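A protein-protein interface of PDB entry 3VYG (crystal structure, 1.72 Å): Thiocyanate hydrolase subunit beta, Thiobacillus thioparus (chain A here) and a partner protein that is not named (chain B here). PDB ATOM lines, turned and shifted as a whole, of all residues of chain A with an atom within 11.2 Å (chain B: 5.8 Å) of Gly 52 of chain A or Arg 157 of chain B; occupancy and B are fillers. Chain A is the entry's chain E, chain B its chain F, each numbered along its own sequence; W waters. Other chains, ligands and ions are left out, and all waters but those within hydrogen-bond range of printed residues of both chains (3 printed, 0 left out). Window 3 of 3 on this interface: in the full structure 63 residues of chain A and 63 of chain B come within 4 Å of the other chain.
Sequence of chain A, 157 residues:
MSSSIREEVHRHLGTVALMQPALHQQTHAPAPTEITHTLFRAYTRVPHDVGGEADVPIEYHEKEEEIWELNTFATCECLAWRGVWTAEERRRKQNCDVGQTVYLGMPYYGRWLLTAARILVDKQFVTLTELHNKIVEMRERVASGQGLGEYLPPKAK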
ATOM      1  N   ARG A  45     -11.577   8.067   3.819  1.00  0.00           N
ATOM      2  CA  ARG A  45     -10.803   9.302   3.649  1.00  0.00           C
ATOM      3  C   ARG A  45     -10.141   9.177   2.289  1.00  0.00           C
ATOM      4  O   ARG A  45      -9.906   8.060   1.790  1.00  0.00           O
ATOM      5  CB  ARG A  45      -9.604   9.319   4.637  1.00  0.00           C
ATOM      6  CG  ARG A  45      -8.548   8.200   4.190  1.00  0.00           C
ATOM      7  CD  ARG A  45      -7.199   8.096   4.939  1.00  0.00           C
ATOM      8  NE  ARG A  45      -6.588   9.407   4.915  1.00  0.00           N
ATOM      9  CZ  ARG A  45      -5.380   9.717   5.351  1.00  0.00           C
ATOM     10  NH1 ARG A  45      -4.552   8.804   5.843  1.00  0.00           N
ATOM     11  NH2 ARG A  45      -5.014  10.965   5.300  1.00  0.00           N
ATOM     12  N   PRO A  47      -6.715   9.286   0.553  1.00  0.00           N
ATOM     13  CA  PRO A  47      -5.378   9.046   1.119  1.00  0.00           C
ATOM     14  C   PRO A  47      -4.446  10.218   0.990  1.00  0.00           C
ATOM     15  O   PRO A  47      -3.515  10.395   1.840  1.00  0.00           O
ATOM     16  CB  PRO A  47      -4.840   7.862   0.270  1.00  0.00           C
ATOM     17  CG  PRO A  47      -6.131   7.173  -0.092  1.00  0.00           C
ATOM     18  CD  PRO A  47      -7.152   8.146  -0.280  1.00  0.00           C
ATOM     19  N   HIS A  48      -4.630  11.009  -0.072  1.00  0.00           N
ATOM     20  CA  HIS A  48      -3.674  12.116  -0.311  1.00  0.00           C
ATOM     21  C   HIS A  48      -3.730  13.201   0.737  1.00  0.00           C
ATOM     22  O   HIS A  48      -2.800  14.039   0.744  1.00  0.00           O
ATOM     23  CB  HIS A  48      -3.799  12.723  -1.748  1.00  0.00           C
ATOM     24  CG  HIS A  48      -5.042  13.544  -1.995  1.00  0.00           C
ATOM     25  ND1 HIS A  48      -5.210  14.215  -3.172  1.00  0.00           N
ATOM     26  CD2 HIS A  48      -6.212  13.700  -1.305  1.00  0.00           C
ATOM     27  CE1 HIS A  48      -6.396  14.803  -3.190  1.00  0.00           C
ATOM     28  NE2 HIS A  48      -7.035  14.507  -2.065  1.00  0.00           N
ATOM     29  N   ASP A  49      -4.808  13.300   1.495  1.00  0.00           N
ATOM     30  CA  ASP A  49      -5.036  14.444   2.396  1.00  0.00           C
ATOM     31  C   ASP A  49      -4.351  14.203   3.790  1.00  0.00           C
ATOM     32  O   ASP A  49      -5.005  13.770   4.764  1.00  0.00           O
ATOM     33  CB  ASP A  49      -6.528  14.636   2.499  1.00  0.00           C
ATOM     34  CG  ASP A  49      -6.963  15.834   3.333  1.00  0.00           C
ATOM     35  OD1 ASP A  49      -6.172  16.737   3.676  1.00  0.00           O
ATOM     36  OD2 ASP A  49      -8.158  15.867   3.601  1.00  0.00           O
ATOM     37  N   VAL A  50      -3.064  14.573   3.836  1.00  0.00           N
ATOM     38  CA  VAL A  50      -2.180  14.166   4.986  1.00  0.00           C
ATOM     39  C   VAL A  50      -1.764  15.381   5.822  1.00  0.00           C
ATOM     40  O   VAL A  50      -1.207  15.180   6.888  1.00  0.00           O
ATOM     41  CB  VAL A  50      -0.935  13.470   4.550  1.00  0.00           C
ATOM     42  CG1 VAL A  50      -1.287  12.133   3.818  1.00  0.00           C
ATOM     43  CG2 VAL A  50       0.117  14.353   3.767  1.00  0.00           C
ATOM     44  N   GLY A  51      -2.157  16.590   5.363  1.00  0.00           N
ATOM     45  CA  GLY A  51      -1.713  17.778   6.112  1.00  0.00           C
ATOM     46  C   GLY A  51      -2.206  17.780   7.550  1.00  0.00           C
ATOM     47  O   GLY A  51      -3.407  17.573   7.867  1.00  0.00           O
ATOM     48  N   GLY A  52      -1.250  18.026   8.457  1.00  0.00           N
ATOM     49  CA  GLY A  52      -1.592  18.130   9.878  1.00  0.00           C
ATOM     50  C   GLY A  52      -1.466  16.814  10.675  1.00  0.00           C
ATOM     51  O   GLY A  52      -1.672  16.776  11.936  1.00  0.00           O
ATOM     52  N   GLU A  53      -1.307  15.689   9.941  1.00  0.00           N
ATOM     53  CA  GLU A  53      -0.966  14.427  10.586  1.00  0.00           C
ATOM     54  C   GLU A  53       0.360  14.537  11.367  1.00  0.00           C
ATOM     55  O   GLU A  53       1.356  15.091  10.918  1.00  0.00           O
ATOM     56  CB  GLU A  53      -0.848  13.312   9.527  1.00  0.00           C
ATOM     57  CG  GLU A  53      -2.240  12.962   9.067  1.00  0.00           C
ATOM     58  CD  GLU A  53      -2.168  11.937   7.942  1.00  0.00           C
ATOM     59  OE1 GLU A  53      -1.145  11.293   7.789  1.00  0.00           O
ATOM     60  OE2 GLU A  53      -3.232  11.745   7.300  1.00  0.00           O
ATOM     61  N   ALA A  54       0.381  13.896  12.550  1.00  0.00           N
ATOM     62  CA  ALA A  54       1.601  13.858  13.351  1.00  0.00           C
ATOM     63  C   ALA A  54       2.678  13.103  12.560  1.00  0.00           C
ATOM     64  O   ALA A  54       2.376  12.053  11.940  1.00  0.00           O
ATOM     65  CB  ALA A  54       1.360  13.084  14.665  1.00  0.00           C
ATOM     66  N   ASP A  55       3.927  13.525  12.681  1.00  0.00           N
ATOM     67  CA  ASP A  55       5.084  12.780  12.137  1.00  0.00           C
ATOM     68  C   ASP A  55       6.331  13.279  12.850  1.00  0.00           C
ATOM     69  O   ASP A  55       6.219  14.249  13.642  1.00  0.00           O
ATOM     70  CB  ASP A  55       5.250  13.024  10.619  1.00  0.00           C
ATOM     71  CG  ASP A  55       5.888  11.853   9.882  1.00  0.00           C
ATOM     72  OD1 ASP A  55       6.660  11.043  10.492  1.00  0.00           O
ATOM     73  OD2 ASP A  55       5.696  11.762   8.604  1.00  0.00           O
ATOM     74  N   VAL A  56       7.394  12.559  12.648  1.00  0.00           N
ATOM     75  CA  VAL A  56       8.657  12.781  13.417  1.00  0.00           C
ATOM     76  C   VAL A  56       9.618  13.585  12.581  1.00  0.00           C
ATOM     77  O   VAL A  56       9.399  13.740  11.379  1.00  0.00           O
ATOM     78  CB  VAL A  56       9.333  11.410  13.807  1.00  0.00           C
ATOM     79  CG1 VAL A  56       8.379  10.551  14.661  1.00  0.00           C
ATOM     80  CG2 VAL A  56       9.875  10.630  12.560  1.00  0.00           C
ATOM     81  N   TYR A  60      16.022  15.269   5.689  1.00  0.00           N
ATOM     82  CA  TYR A  60      15.517  15.373   4.254  1.00  0.00           C
ATOM     83  C   TYR A  60      16.646  15.142   3.340  1.00  0.00           C
ATOM     84  O   TYR A  60      17.764  15.679   3.499  1.00  0.00           O
ATOM     85  CB  TYR A  60      14.861  16.748   4.106  1.00  0.00           C
ATOM     86  CG  TYR A  60      13.569  16.872   4.771  1.00  0.00           C
ATOM     87  CD1 TYR A  60      12.551  15.970   4.607  1.00  0.00           C
ATOM     88  CD2 TYR A  60      13.271  18.008   5.564  1.00  0.00           C
ATOM     89  CE1 TYR A  60      11.315  16.172   5.215  1.00  0.00           C
ATOM     90  CE2 TYR A  60      12.040  18.161   6.247  1.00  0.00           C
ATOM     91  CZ  TYR A  60      11.037  17.247   6.004  1.00  0.00           C
ATOM     92  OH  TYR A  60       9.844  17.454   6.631  1.00  0.00           O
ATOM     93  N   ARG B 152       4.834  17.068   3.742  1.00  0.00           N
ATOM     94  CA  ARG B 152       3.445  17.341   3.464  1.00  0.00           C
ATOM     95  C   ARG B 152       2.557  17.306   4.711  1.00  0.00           C
ATOM     96  O   ARG B 152       1.563  18.027   4.780  1.00  0.00           O
ATOM     97  CB  ARG B 152       3.037  16.316   2.408  1.00  0.00           C
ATOM     98  CG  ARG B 152       3.611  16.634   1.126  1.00  0.00           C
ATOM     99  CD  ARG B 152       3.386  15.466   0.067  1.00  0.00           C
ATOM    100  NE  ARG B 152       1.964  15.166   0.021  1.00  0.00           N
ATOM    101  CZ  ARG B 152       1.413  13.941   0.043  1.00  0.00           C
ATOM    102  NH1 ARG B 152       2.186  12.883  -0.193  1.00  0.00           N
ATOM    103  NH2 ARG B 152       0.126  13.795   0.122  1.00  0.00           N
ATOM    104  N   ARG B 153       2.877  16.419   5.687  1.00  0.00           N
ATOM    105  CA  ARG B 153       2.127  16.427   6.957  1.00  0.00           C
ATOM    106  C   ARG B 153       2.512  17.627   7.837  1.00  0.00           C
ATOM    107  O   ARG B 153       1.657  18.169   8.497  1.00  0.00           O
ATOM    108  CB  ARG B 153       2.461  15.110   7.767  1.00  0.00           C
ATOM    109  CG  ARG B 153       1.830  13.824   7.043  1.00  0.00           C
ATOM    110  CD  ARG B 153       2.409  12.583   7.802  1.00  0.00           C
ATOM    111  NE  ARG B 153       1.722  11.350   7.292  1.00  0.00           N
ATOM    112  CZ  ARG B 153       2.377  10.255   7.011  1.00  0.00           C
ATOM    113  NH1 ARG B 153       3.709  10.206   7.180  1.00  0.00           N
ATOM    114  NH2 ARG B 153       1.678   9.194   6.497  1.00  0.00           N
ATOM    115  N   ARG B 154       3.802  17.862   7.991  1.00  0.00           N
ATOM    116  CA  ARG B 154       4.260  18.672   9.128  1.00  0.00           C
ATOM    117  C   ARG B 154       4.351  20.175   8.835  1.00  0.00           C
ATOM    118  O   ARG B 154       4.052  20.938   9.706  1.00  0.00           O
ATOM    119  CB  ARG B 154       5.681  18.224   9.533  1.00  0.00           C
ATOM    120  CG  ARG B 154       5.675  16.819  10.103  1.00  0.00           C
ATOM    121  CD  ARG B 154       6.965  16.629  10.972  1.00  0.00           C
ATOM    122  NE  ARG B 154       8.125  16.763  10.138  1.00  0.00           N
ATOM    123  CZ  ARG B 154       9.332  17.220  10.544  1.00  0.00           C
ATOM    124  NH1 ARG B 154       9.508  17.587  11.861  1.00  0.00           N
ATOM    125  NH2 ARG B 154      10.317  17.389   9.699  1.00  0.00           N
ATOM    126  N   LEU B 155       4.697  20.577   7.637  1.00  0.00           N
ATOM    127  CA  LEU B 155       4.886  22.039   7.444  1.00  0.00           C
ATOM    128  C   LEU B 155       3.673  22.855   7.750  1.00  0.00           C
ATOM    129  O   LEU B 155       3.791  23.929   8.370  1.00  0.00           O
ATOM    130  CB  LEU B 155       5.302  22.334   6.008  1.00  0.00           C
ATOM    131  CG  LEU B 155       5.691  23.789   5.707  1.00  0.00           C
ATOM    132  CD1 LEU B 155       7.128  24.064   6.322  1.00  0.00           C
ATOM    133  CD2 LEU B 155       5.720  24.168   4.197  1.00  0.00           C
ATOM    134  N   VAL B 156       2.459  22.438   7.354  1.00  0.00           N
ATOM    135  CA  VAL B 156       1.299  23.282   7.560  1.00  0.00           C
ATOM    136  C   VAL B 156       1.007  23.515   9.083  1.00  0.00           C
ATOM    137  O   VAL B 156       0.318  24.437   9.427  1.00  0.00           O
ATOM    138  CB  VAL B 156      -0.031  22.688   6.945  1.00  0.00           C
ATOM    139  CG1 VAL B 156       0.062  22.840   5.423  1.00  0.00           C
ATOM    140  CG2 VAL B 156      -0.264  21.170   7.277  1.00  0.00           C
ATOM    141  N   ARG B 157       1.415  22.546   9.933  1.00  0.00           N
ATOM    142  CA  ARG B 157       1.057  22.543  11.345  1.00  0.00           C
ATOM    143  C   ARG B 157       2.211  22.971  12.283  1.00  0.00           C
ATOM    144  O   ARG B 157       1.901  23.608  13.326  1.00  0.00           O
ATOM    145  CB  ARG B 157       0.518  21.148  11.749  1.00  0.00           C
ATOM    146  CG  ARG B 157      -0.015  21.107  13.211  1.00  0.00           C
ATOM    147  CD  ARG B 157      -0.730  19.764  13.387  1.00  0.00           C
ATOM    148  NE  ARG B 157      -1.348  19.689  14.735  1.00  0.00           N
ATOM    149  CZ  ARG B 157      -2.452  18.975  15.025  1.00  0.00           C
ATOM    150  NH1 ARG B 157      -2.981  18.081  14.141  1.00  0.00           N
ATOM    151  NH2 ARG B 157      -3.002  19.105  16.260  1.00  0.00           N
ATOM    152  N   TRP B 158       3.406  22.617  11.952  1.00  0.00           N
ATOM    153  CA  TRP B 158       4.601  23.002  12.735  1.00  0.00           C
ATOM    154  C   TRP B 158       5.608  23.659  11.845  1.00  0.00           C
ATOM    155  O   TRP B 158       6.756  23.214  11.783  1.00  0.00           O
ATOM    156  CB  TRP B 158       5.188  21.702  13.394  1.00  0.00           C
ATOM    157  CG  TRP B 158       4.216  20.954  14.291  1.00  0.00           C
ATOM    158  CD1 TRP B 158       3.849  21.246  15.577  1.00  0.00           C
ATOM    159  CD2 TRP B 158       3.501  19.773  13.922  1.00  0.00           C
ATOM    160  NE1 TRP B 158       2.915  20.324  16.034  1.00  0.00           N
ATOM    161  CE2 TRP B 158       2.725  19.389  15.042  1.00  0.00           C
ATOM    162  CE3 TRP B 158       3.449  19.012  12.719  1.00  0.00           C
ATOM    163  CZ2 TRP B 158       1.911  18.278  15.025  1.00  0.00           C
ATOM    164  CZ3 TRP B 158       2.649  17.863  12.703  1.00  0.00           C
ATOM    165  CH2 TRP B 158       1.868  17.537  13.837  1.00  0.00           C
ATOM    166  N   PRO B 159       5.262  24.765  11.182  1.00  0.00           N
ATOM    167  CA  PRO B 159       6.218  25.269  10.253  1.00  0.00           C
ATOM    168  C   PRO B 159       7.481  25.775  10.906  1.00  0.00           C
ATOM    169  O   PRO B 159       8.574  25.669  10.349  1.00  0.00           O
ATOM    170  CB  PRO B 159       5.478  26.454   9.543  1.00  0.00           C
ATOM    171  CG  PRO B 159       4.355  26.858  10.533  1.00  0.00           C
ATOM    172  CD  PRO B 159       3.941  25.449  11.139  1.00  0.00           C
HETATM  173  O   HOH W   1       3.427   9.926  10.488  1.00  0.00           O
HETATM  174  O   HOH W   2       7.840  16.443  14.180  1.00  0.00           O
HETATM  175  O   HOH W   3      -1.355   9.177   6.085  1.00  0.00           O
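The side-chain carboxylate of Glu 53 of chain A is in salt-bridge range of the guanidinium group of Arg 45 of chain A (2.8 Å).
Arg 45 of chain A touches none of the printed residues of chain B. Asp 49 of chain A touches none of the printed residues of chain B. Printed residues of chain B within 4 Å of Val 50 of chain A: Arg 152 (3.7 Å) and Arg 153 (3.3 Å). Of chain B, only Arg 153, Val 156 and Arg 157 come within 4 Å of Gly 52 of chain A. Printed residues of chain B within 4 Å of Ala 54 of chain A: Trp 158. Of the printed residues of chain B, Asp 55 of chain A touches Arg 153 (2.9 Å) and Arg 154 (3.7 Å). Of the printed residues of chain B, Val 56 of chain A touches Arg 154. Of the printed residues of chain A, Arg 153 of chain B touches Val 50 (3.3 Å), Gly 51 (3.996 Å), Gly 52 (2.9 Å), Glu 53 (2.9 Å) and Asp 55 (2.9 Å). Val 156 of chain B touches two residues of chain A. Printed residues of chain A within 4 Å of Arg 157 of chain B: Gly 52. Trp 158 of chain B touches just these residues of chain A: Glu 53 and Ala 54. The nearest residue of chain B that does not touch Gly 52 of chain A is Trp 158 of chain B (4.1 Å).
Among the printed residues, pairs that only touch across the chains: Val 50 of chain A with Arg 153 of chain B (3.3 Å), Gly 52 of chain A with Val 156 of chain B (3.5 Å), Val 56 of chain A with Arg 154 of chain B (3.5 Å), Glu 53 of chain A with Trp 158 of chain B (3.5 Å), Gly 51 of chain A with Arg 152 of chain B (3.5 Å), Asp 55 of chain A with Arg 154 of chain B (3.7 Å), Val 50 of chain A with Arg 152 of chain B (3.7 Å), Ala 54 of chain A with Trp 158 of chain B (3.7 Å), Gly 51 of chain A with Val 156 of chain B (3.9 Å) and Gly 51 of chain A with Arg 153 of chain B (3.996 Å).
Printed residues of chain A that touch a printed residue of chain B: His 48, Val 50, Gly 51, Gly 52, Glu 53, Ala 54, Asp 55, Val 56 and Tyr 60. Hydrophobic or aromatic side chains of chain A that line the printed part of chain B: Val 50 and Tyr 60. Of the 8 printed residues of chain B, 6 touch a printed residue of chain A. Hydrophobic or aromatic side chains of chain B that line the printed part of chain A: Val 156 and Trp 158. Among the printed residues, Asp or Glu carboxylates within 4 Å of a Lys or Arg side-chain nitrogen of the other chain: Glu 53 of chain A with Arg 153 of chain B (2.9 Å) and Asp 55 of chain A with Arg 153 of chain B (2.9 Å).
Water W3 lies within hydrogen-bond range of the side-chain carboxylate of Glu 53 of chain A (2.7 Å), the guanidinium group of Arg 153 of chain B (3.1 Å) and the guanidinium group of Arg 45 of chain A (3.2 Å). Water W2 bridges the backbone carbonyl oxygen of Asp 55 of chain A (2.8 Å) and the guanidinium group of Arg 154 of chain B (3.1 Å). Water W1 lies within hydrogen-bond range of O of Ala 54 of chain A (2.8 Å), NH1 of Arg 153 of chain B (3.3 Å) and OD1 of Asp 55 of chain A (3.4 Å).
The guanidinium group (NH2) of Arg 152 of chain B sits at hydrogen-bond distance from the backbone carbonyl oxygen (O) of His 48 of chain A. The backbone carbonyl oxygen (O) of Arg 153 of chain B sits at hydrogen-bond distance from the backbone NH (N) of Gly 52 of chain A (2.9 Å). O of Gly 52 of chain A lies within hydrogen-bond range of NH1 of Arg 157 of chain B (2.9 Å). The guanidinium group (NE) of Arg 153 of chain B lies within salt-bridge range of the side-chain carboxylate (OE1) of Glu 53 of chain A (2.9 Å). The guanidinium group (NH1) of Arg 153 of chain B is in salt-bridge range of the side-chain carboxylate (OD2) of Asp 55 of chain A (2.9 Å). The guanidinium group (NH2) of Arg 154 of chain B lies within hydrogen-bond range of the side-chain hydroxyl (OH) of Tyr 60 of chain A, 3.1 Å away.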
